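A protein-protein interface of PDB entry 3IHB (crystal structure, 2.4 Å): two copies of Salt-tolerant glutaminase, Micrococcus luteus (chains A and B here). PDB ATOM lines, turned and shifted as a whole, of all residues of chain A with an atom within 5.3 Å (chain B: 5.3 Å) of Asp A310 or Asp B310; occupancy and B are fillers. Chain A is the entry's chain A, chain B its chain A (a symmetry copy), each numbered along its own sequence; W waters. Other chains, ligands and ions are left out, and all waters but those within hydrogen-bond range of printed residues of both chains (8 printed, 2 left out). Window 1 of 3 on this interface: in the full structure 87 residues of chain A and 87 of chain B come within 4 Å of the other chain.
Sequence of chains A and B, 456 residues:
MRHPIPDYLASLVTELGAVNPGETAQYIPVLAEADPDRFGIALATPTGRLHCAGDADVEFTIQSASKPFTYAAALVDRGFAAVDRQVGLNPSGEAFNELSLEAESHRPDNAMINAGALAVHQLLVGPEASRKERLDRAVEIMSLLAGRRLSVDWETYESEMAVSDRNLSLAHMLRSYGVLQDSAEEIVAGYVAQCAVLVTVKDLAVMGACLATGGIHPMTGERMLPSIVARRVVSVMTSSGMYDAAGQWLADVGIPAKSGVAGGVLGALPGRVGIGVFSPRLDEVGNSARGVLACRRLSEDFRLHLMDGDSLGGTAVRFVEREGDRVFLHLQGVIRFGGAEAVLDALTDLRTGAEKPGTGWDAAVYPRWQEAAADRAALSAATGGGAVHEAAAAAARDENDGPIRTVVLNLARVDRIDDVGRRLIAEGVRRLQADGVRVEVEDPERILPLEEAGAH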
ATOM      1  N   GLY A 271      22.961 -23.867  -5.514  1.00  0.00           N
ATOM      2  CA  GLY A 271      22.634 -22.941  -4.449  1.00  0.00           C
ATOM      3  C   GLY A 271      22.422 -21.483  -4.832  1.00  0.00           C
ATOM      4  O   GLY A 271      21.986 -20.691  -3.999  1.00  0.00           O
ATOM      5  N   ARG A 272      22.696 -21.107  -6.075  1.00  0.00           N
ATOM      6  CA  ARG A 272      22.548 -19.703  -6.446  1.00  0.00           C
ATOM      7  C   ARG A 272      21.668 -19.323  -7.630  1.00  0.00           C
ATOM      8  O   ARG A 272      20.854 -18.417  -7.497  1.00  0.00           O
ATOM      9  CB  ARG A 272      23.940 -19.065  -6.615  1.00  0.00           C
ATOM     10  CG  ARG A 272      24.709 -18.943  -5.295  1.00  0.00           C
ATOM     11  CD  ARG A 272      26.104 -19.532  -5.382  1.00  0.00           C
ATOM     12  NE  ARG A 272      27.112 -18.524  -5.687  1.00  0.00           N
ATOM     13  CZ  ARG A 272      28.385 -18.795  -5.965  1.00  0.00           C
ATOM     14  NH1 ARG A 272      28.820 -20.053  -5.984  1.00  0.00           N
ATOM     15  NH2 ARG A 272      29.231 -17.803  -6.223  1.00  0.00           N
ATOM     16  N   ASP A 308      33.769 -19.331  -5.918  1.00  0.00           N
ATOM     17  CA  ASP A 308      33.587 -18.203  -5.014  1.00  0.00           C
ATOM     18  C   ASP A 308      32.534 -18.669  -4.024  1.00  0.00           C
ATOM     19  O   ASP A 308      31.339 -18.671  -4.320  1.00  0.00           O
ATOM     20  CB  ASP A 308      33.120 -16.960  -5.787  1.00  0.00           C
ATOM     21  CG  ASP A 308      34.283 -16.177  -6.385  1.00  0.00           C
ATOM     22  OD1 ASP A 308      34.183 -15.696  -7.535  1.00  0.00           O
ATOM     23  OD2 ASP A 308      35.304 -16.034  -5.690  1.00  0.00           O
ATOM     24  N   GLY A 309      33.000 -19.093  -2.855  1.00  0.00           N
ATOM     25  CA  GLY A 309      32.115 -19.610  -1.827  1.00  0.00           C
ATOM     26  C   GLY A 309      31.040 -18.693  -1.277  1.00  0.00           C
ATOM     27  O   GLY A 309      31.254 -17.500  -1.082  1.00  0.00           O
ATOM     28  N   ASP A 310      29.872 -19.271  -1.021  1.00  0.00           N
ATOM     29  CA  ASP A 310      28.737 -18.545  -0.470  1.00  0.00           C
ATOM     30  C   ASP A 310      28.050 -19.518   0.491  1.00  0.00           C
ATOM     31  O   ASP A 310      27.002 -20.081   0.185  1.00  0.00           O
ATOM     32  CB  ASP A 310      27.787 -18.143  -1.594  1.00  0.00           C
ATOM     33  CG  ASP A 310      26.774 -17.115  -1.156  1.00  0.00           C
ATOM     34  OD1 ASP A 310      27.185 -15.985  -0.827  1.00  0.00           O
ATOM     35  OD2 ASP A 310      25.568 -17.429  -1.141  1.00  0.00           O
ATOM     36  N   SER A 311      28.650 -19.711   1.658  1.00  0.00           N
ATOM     37  CA  SER A 311      28.122 -20.657   2.636  1.00  0.00           C
ATOM     38  C   SER A 311      27.354 -20.011   3.787  1.00  0.00           C
ATOM     39  O   SER A 311      27.567 -18.844   4.099  1.00  0.00           O
ATOM     40  CB  SER A 311      29.283 -21.495   3.182  1.00  0.00           C
ATOM     41  OG  SER A 311      28.831 -22.549   4.009  1.00  0.00           O
ATOM     42  N   LEU A 312      26.454 -20.773   4.410  1.00  0.00           N
ATOM     43  CA  LEU A 312      25.672 -20.268   5.538  1.00  0.00           C
ATOM     44  C   LEU A 312      26.586 -20.018   6.746  1.00  0.00           C
ATOM     45  O   LEU A 312      26.454 -19.002   7.444  1.00  0.00           O
ATOM     46  CB  LEU A 312      24.562 -21.259   5.917  1.00  0.00           C
ATOM     47  CG  LEU A 312      23.729 -20.904   7.165  1.00  0.00           C
ATOM     48  CD1 LEU A 312      23.138 -19.502   7.015  1.00  0.00           C
ATOM     49  CD2 LEU A 312      22.614 -21.926   7.367  1.00  0.00           C
ATOM     50  N   GLY A 313      27.508 -20.951   6.980  1.00  0.00           N
ATOM     51  CA  GLY A 313      28.452 -20.826   8.075  1.00  0.00           C
ATOM     52  C   GLY A 313      27.854 -20.640   9.457  1.00  0.00           C
ATOM     53  O   GLY A 313      26.811 -21.207   9.786  1.00  0.00           O
ATOM     54  N   VAL A 334      18.959 -22.855   5.875  1.00  0.00           N
ATOM     55  CA  VAL A 334      18.941 -24.234   5.392  1.00  0.00           C
ATOM     56  C   VAL A 334      20.167 -24.899   6.004  1.00  0.00           C
ATOM     57  O   VAL A 334      21.301 -24.634   5.591  1.00  0.00           O
ATOM     58  CB  VAL A 334      19.050 -24.285   3.863  1.00  0.00           C
ATOM     59  CG1 VAL A 334      19.097 -25.722   3.391  1.00  0.00           C
ATOM     60  CG2 VAL A 334      17.873 -23.555   3.250  1.00  0.00           C
ATOM     61  N   ARG A 336      22.813 -27.716   6.707  1.00  0.00           N
ATOM     62  CA  ARG A 336      23.464 -28.881   6.137  1.00  0.00           C
ATOM     63  C   ARG A 336      24.738 -29.013   6.956  1.00  0.00           C
ATOM     64  O   ARG A 336      24.817 -28.486   8.066  1.00  0.00           O
ATOM     65  CB  ARG A 336      23.801 -28.651   4.656  1.00  0.00           C
ATOM     66  CG  ARG A 336      22.586 -28.349   3.787  1.00  0.00           C
ATOM     67  CD  ARG A 336      22.921 -28.364   2.301  1.00  0.00           C
ATOM     68  NE  ARG A 336      23.175 -29.717   1.805  1.00  0.00           N
ATOM     69  CZ  ARG A 336      23.511 -30.011   0.552  1.00  0.00           C
ATOM     70  NH1 ARG A 336      23.640 -29.048  -0.347  1.00  0.00           N
ATOM     71  NH2 ARG A 336      23.715 -31.273   0.193  1.00  0.00           N
ATOM     72  N   PHE A 337      25.733 -29.702   6.424  1.00  0.00           N
ATOM     73  CA  PHE A 337      26.973 -29.857   7.157  1.00  0.00           C
ATOM     74  C   PHE A 337      27.526 -28.506   7.607  1.00  0.00           C
ATOM     75  O   PHE A 337      28.042 -28.369   8.722  1.00  0.00           O
ATOM     76  CB  PHE A 337      28.025 -30.549   6.294  1.00  0.00           C
ATOM     77  CG  PHE A 337      29.323 -30.742   7.001  1.00  0.00           C
ATOM     78  CD1 PHE A 337      29.542 -31.874   7.779  1.00  0.00           C
ATOM     79  CD2 PHE A 337      30.307 -29.759   6.950  1.00  0.00           C
ATOM     80  CE1 PHE A 337      30.719 -32.023   8.495  1.00  0.00           C
ATOM     81  CE2 PHE A 337      31.487 -29.901   7.663  1.00  0.00           C
ATOM     82  CZ  PHE A 337      31.696 -31.032   8.435  1.00  0.00           C
ATOM     83  N   GLY A 338      27.429 -27.513   6.729  1.00  0.00           N
ATOM     84  CA  GLY A 338      27.943 -26.190   7.045  1.00  0.00           C
ATOM     85  C   GLY A 338      27.380 -25.623   8.328  1.00  0.00           C
ATOM     86  O   GLY A 338      28.128 -25.265   9.239  1.00  0.00           O
ATOM     87  N   GLY A 339      26.057 -25.543   8.401  1.00  0.00           N
ATOM     88  CA  GLY A 339      25.415 -25.019   9.591  1.00  0.00           C
ATOM     89  C   GLY A 339      25.527 -25.977  10.758  1.00  0.00           C
ATOM     90  O   GLY A 339      25.893 -25.576  11.861  1.00  0.00           O
ATOM     91  N   GLY B 271      34.246 -22.011   0.792  1.00  0.00           N
ATOM     92  CA  GLY B 271      33.225 -21.701   1.774  1.00  0.00           C
ATOM     93  C   GLY B 271      32.971 -22.732   2.865  1.00  0.00           C
ATOM     94  O   GLY B 271      32.236 -22.450   3.810  1.00  0.00           O
ATOM     95  N   ARG B 272      33.572 -23.911   2.778  1.00  0.00           N
ATOM     96  CA  ARG B 272      33.300 -24.929   3.788  1.00  0.00           C
ATOM     97  C   ARG B 272      34.454 -25.561   4.554  1.00  0.00           C
ATOM     98  O   ARG B 272      34.378 -25.650   5.774  1.00  0.00           O
ATOM     99  CB  ARG B 272      32.420 -26.037   3.178  1.00  0.00           C
ATOM    100  CG  ARG B 272      31.001 -25.563   2.846  1.00  0.00           C
ATOM    101  CD  ARG B 272      30.602 -25.888   1.419  1.00  0.00           C
ATOM    102  NE  ARG B 272      29.858 -27.138   1.324  1.00  0.00           N
ATOM    103  CZ  ARG B 272      29.522 -27.727   0.178  1.00  0.00           C
ATOM    104  NH1 ARG B 272      29.867 -27.184  -0.987  1.00  0.00           N
ATOM    105  NH2 ARG B 272      28.834 -28.864   0.196  1.00  0.00           N
ATOM    106  N   ASP B 308      26.935 -29.758  -4.118  1.00  0.00           N
ATOM    107  CA  ASP B 308      25.869 -29.740  -3.125  1.00  0.00           C
ATOM    108  C   ASP B 308      25.896 -28.332  -2.557  1.00  0.00           C
ATOM    109  O   ASP B 308      26.732 -28.002  -1.716  1.00  0.00           O
ATOM    110  CB  ASP B 308      26.127 -30.791  -2.036  1.00  0.00           C
ATOM    111  CG  ASP B 308      25.616 -32.173  -2.428  1.00  0.00           C
ATOM    112  OD1 ASP B 308      26.297 -33.187  -2.161  1.00  0.00           O
ATOM    113  OD2 ASP B 308      24.515 -32.243  -3.001  1.00  0.00           O
ATOM    114  N   GLY B 309      24.985 -27.501  -3.051  1.00  0.00           N
ATOM    115  CA  GLY B 309      24.920 -26.112  -2.636  1.00  0.00           C
ATOM    116  C   GLY B 309      24.669 -25.812  -1.170  1.00  0.00           C
ATOM    117  O   GLY B 309      23.888 -26.484  -0.504  1.00  0.00           O
ATOM    118  N   ASP B 310      25.342 -24.780  -0.675  1.00  0.00           N
ATOM    119  CA  ASP B 310      25.206 -24.339   0.706  1.00  0.00           C
ATOM    120  C   ASP B 310      25.288 -22.812   0.663  1.00  0.00           C
ATOM    121  O   ASP B 310      26.304 -22.219   1.017  1.00  0.00           O
ATOM    122  CB  ASP B 310      26.344 -24.913   1.545  1.00  0.00           C
ATOM    123  CG  ASP B 310      26.093 -24.782   3.027  1.00  0.00           C
ATOM    124  OD1 ASP B 310      25.139 -25.413   3.522  1.00  0.00           O
ATOM    125  OD2 ASP B 310      26.845 -24.052   3.700  1.00  0.00           O
ATOM    126  N   SER B 311      24.209 -22.178   0.224  1.00  0.00           N
ATOM    127  CA  SER B 311      24.185 -20.726   0.086  1.00  0.00           C
ATOM    128  C   SER B 311      23.454 -19.996   1.211  1.00  0.00           C
ATOM    129  O   SER B 311      22.599 -20.574   1.874  1.00  0.00           O
ATOM    130  CB  SER B 311      23.553 -20.374  -1.266  1.00  0.00           C
ATOM    131  OG  SER B 311      23.649 -18.993  -1.551  1.00  0.00           O
ATOM    132  N   LEU B 312      23.801 -18.727   1.428  1.00  0.00           N
ATOM    133  CA  LEU B 312      23.157 -17.923   2.467  1.00  0.00           C
ATOM    134  C   LEU B 312      21.688 -17.665   2.101  1.00  0.00           C
ATOM    135  O   LEU B 312      20.797 -17.741   2.958  1.00  0.00           O
ATOM    136  CB  LEU B 312      23.893 -16.589   2.656  1.00  0.00           C
ATOM    137  CG  LEU B 312      23.254 -15.594   3.644  1.00  0.00           C
ATOM    138  CD1 LEU B 312      23.050 -16.266   5.002  1.00  0.00           C
ATOM    139  CD2 LEU B 312      24.135 -14.357   3.797  1.00  0.00           C
ATOM    140  N   GLY B 313      21.453 -17.361   0.825  1.00  0.00           N
ATOM    141  CA  GLY B 313      20.106 -17.117   0.341  1.00  0.00           C
ATOM    142  C   GLY B 313      19.322 -16.034   1.059  1.00  0.00           C
ATOM    143  O   GLY B 313      19.872 -15.015   1.479  1.00  0.00           O
ATOM    144  N   VAL B 334      27.533 -13.192   5.682  1.00  0.00           N
ATOM    145  CA  VAL B 334      28.505 -12.689   4.713  1.00  0.00           C
ATOM    146  C   VAL B 334      27.716 -12.424   3.437  1.00  0.00           C
ATOM    147  O   VAL B 334      27.314 -13.361   2.739  1.00  0.00           O
ATOM    148  CB  VAL B 334      29.591 -13.734   4.428  1.00  0.00           C
ATOM    149  CG1 VAL B 334      30.548 -13.218   3.375  1.00  0.00           C
ATOM    150  CG2 VAL B 334      30.327 -14.059   5.711  1.00  0.00           C
ATOM    151  N   ARG B 336      27.076 -11.448  -0.313  1.00  0.00           N
ATOM    152  CA  ARG B 336      27.671 -11.427  -1.636  1.00  0.00           C
ATOM    153  C   ARG B 336      26.470 -11.362  -2.565  1.00  0.00           C
ATOM    154  O   ARG B 336      25.383 -10.964  -2.145  1.00  0.00           O
ATOM    155  CB  ARG B 336      28.479 -12.707  -1.894  1.00  0.00           C
ATOM    156  CG  ARG B 336      29.611 -12.933  -0.900  1.00  0.00           C
ATOM    157  CD  ARG B 336      30.533 -14.071  -1.322  1.00  0.00           C
ATOM    158  NE  ARG B 336      31.363 -13.713  -2.473  1.00  0.00           N
ATOM    159  CZ  ARG B 336      32.236 -14.529  -3.057  1.00  0.00           C
ATOM    160  NH1 ARG B 336      32.401 -15.762  -2.605  1.00  0.00           N
ATOM    161  NH2 ARG B 336      32.952 -14.110  -4.094  1.00  0.00           N
ATOM    162  N   PHE B 337      26.649 -11.750  -3.817  1.00  0.00           N
ATOM    163  CA  PHE B 337      25.539 -11.713  -4.746  1.00  0.00           C
ATOM    164  C   PHE B 337      24.325 -12.459  -4.193  1.00  0.00           C
ATOM    165  O   PHE B 337      23.181 -12.019  -4.353  1.00  0.00           O
ATOM    166  CB  PHE B 337      25.931 -12.347  -6.078  1.00  0.00           C
ATOM    167  CG  PHE B 337      24.826 -12.331  -7.079  1.00  0.00           C
ATOM    168  CD1 PHE B 337      24.644 -11.233  -7.913  1.00  0.00           C
ATOM    169  CD2 PHE B 337      23.920 -13.385  -7.145  1.00  0.00           C
ATOM    170  CE1 PHE B 337      23.576 -11.184  -8.794  1.00  0.00           C
ATOM    171  CE2 PHE B 337      22.849 -13.344  -8.023  1.00  0.00           C
ATOM    172  CZ  PHE B 337      22.675 -12.245  -8.850  1.00  0.00           C
ATOM    173  N   GLY B 338      24.579 -13.595  -3.554  1.00  0.00           N
ATOM    174  CA  GLY B 338      23.497 -14.397  -3.006  1.00  0.00           C
ATOM    175  C   GLY B 338      22.598 -13.623  -2.068  1.00  0.00           C
ATOM    176  O   GLY B 338      21.385 -13.554  -2.273  1.00  0.00           O
ATOM    177  N   GLY B 339      23.194 -13.035  -1.038  1.00  0.00           N
ATOM    178  CA  GLY B 339      22.425 -12.264  -0.082  1.00  0.00           C
ATOM    179  C   GLY B 339      21.935 -10.961  -0.677  1.00  0.00           C
ATOM    180  O   GLY B 339      20.760 -10.619  -0.551  1.00  0.00           O
HETATM  181  O   HOH W   1      24.298 -25.166   6.192  1.00  0.00           O
HETATM  182  O   HOH W   2      25.556 -13.966   0.255  1.00  0.00           O
HETATM  183  O   HOH W   3      20.198 -20.629   4.446  1.00  0.00           O
HETATM  184  O   HOH W   4      21.231 -18.081  -3.368  1.00  0.00           O
HETATM  185  O   HOH W   5      27.390 -27.199   4.093  1.00  0.00           O
HETATM  186  O   HOH W   6      26.952 -16.022   6.109  1.00  0.00           O
HETATM  187  O   HOH W   7      31.011 -23.243   6.187  1.00  0.00           O
HETATM  188  O   HOH W   8      26.390 -15.536  -3.610  1.00  0.00           O
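O of Asp A310 sits close to O of Asp B310, at 2.4 Å.
The backbone NH (N) of Leu A312 is in hydrogen-bond range of the side-chain carboxylate (OD2) of Asp B310 (3.4 Å).
NH1 of Arg A336 sits at hydrogen-bond distance from O of Gly B309, at 2.6 Å.
The side-chain hydroxyl of Ser B311 sits close to the backbone carbonyl oxygen of Gly A271 (3.4 Å).
The side-chain hydroxyl (OG) of Ser B311 sits at hydrogen-bond distance from the side-chain carboxylate (OD2) of Asp A310 (2.5 Å).
The side-chain carboxylate (OD2) of Asp A310 is in hydrogen-bond range of the backbone NH (N) of Leu B312 (3.4 Å).
NH2 of Arg B336 is in salt-bridge range of OD2 of Asp A308 (3.4 Å).
O of Gly A309 lies within hydrogen-bond range of NH1 of Arg B336, 2.6 Å away.
The backbone carbonyl oxygen (O) of Gly B271 lies close to the side-chain hydroxyl (OG) of Ser A311 (3.4 Å).
OD2 of Asp B308 lies within salt-bridge range of NH2 of Arg A336, at 3.4 Å.
The side-chain carboxylate (OD2) of Asp B310 is in hydrogen-bond range of the side-chain hydroxyl (OG) of Ser A311 (2.5 Å).
The backbone carbonyl oxygen (O) of Asp B308 lies within hydrogen-bond range of the guanidinium group (NH2) of Arg B272 (3.0 Å).
NH2 of Arg A272 is in hydrogen-bond range of O of Asp A308, at 3.0 Å.
Among the printed residues, merely in contact across the chains: Asp A310 with Arg B336, Arg A336 with Asp B310, Leu A312 with Leu B312, Arg A272 with Ser B311 and Ser A311 with Arg B272.
Asp A310 touches just these residues of chain B: Asp B310 (2.4 Å), Ser B311 (2.5 Å), Leu B312 (3.4 Å) and Arg B336 (3.7 Å).
Of chain A, only Asp A310 (2.4 Å), Ser A311 (2.5 Å), Leu A312 (3.4 Å) and Arg A336 (3.7 Å) come within 4 Å of Asp B310.
Of the printed residues of chain B, Ser A311 touches Gly B271, Arg B272 and Asp B310.
Printed residues of chain B within 4 Å of Gly A309: Arg B336.
Of the printed residues of chain A, Gly B309 touches Arg A336.
Of the printed residues of chain B, Arg A336 touches Asp B308 (3.2 Å), Gly B309 (2.6 Å) and Asp B310 (3.7 Å).
Of the printed residues of chain B, Asp A308 touches Arg B336.
Gly B313 touches none of the printed residues of chain A.
Gly B339 touches none of the printed residues of chain A.
The nearest residue of chain A that does not touch Asp B310 is Gly A338 (4.1 Å).
The nearest printed residue of chain B that does not touch Gly A271 is Gly B309 (4.1 Å).
Of the 13 printed residues of chain B, 8 touch a printed residue of chain A.
Hydrophobic or aromatic side chains of chain B within 4 Å of the printed part of chain A: Leu B312.
Of the 13 printed residues of chain A, 8 touch a printed residue of chain B.
Among the printed residues, 16 pairs touch across the chains.
Among the printed residues, Asp or Glu carboxylates within 4 Å of a Lys or Arg side-chain nitrogen of the other chain: Asp A308 with Arg B336 (3.4 Å) and Arg A336 with Asp B308 (3.4 Å).
Arg A272 touches Ser B311, and with the chains exchanged Ser A311 touches Arg B272.
Asp A308 touches Arg B336, and with the chains exchanged Arg A336 touches Asp B308.
Gly A309 touches Arg B336, and with the chains exchanged Arg A336 touches Gly B309.
Asp A310 touches Ser B311, and with the chains exchanged Ser A311 touches Asp B310.
Of the 16 pairs that touch across the chains among the printed residues, 16 have their exchanged pair printed and touching as well.
Water W8 lies within hydrogen-bond range of N of Gly B338 (2.7 Å) and OD1 of Asp A310 (2.9 Å).
Water W5 lies within hydrogen-bond range of N of Gly A338 (2.7 Å) and OD1 of Asp B310 (2.9 Å).
Water W4 bridges O of Gly A271 (2.8 Å) and OG of Ser B311 (3.2 Å).
Water W2 lies within hydrogen-bond range of the side-chain carboxylate of Asp A310, the backbone NH of Gly B339, the backbone NH of Arg B336 and the backbone carbonyl oxygen of Val B334.
Water W6 lies within hydrogen-bond range of the backbone NH of Val B334 (2.9 Å) and the backbone carbonyl oxygen of Leu A312 (3.3 Å).
Water W3 lies within hydrogen-bond range of N of Val A334 and O of Leu B312.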
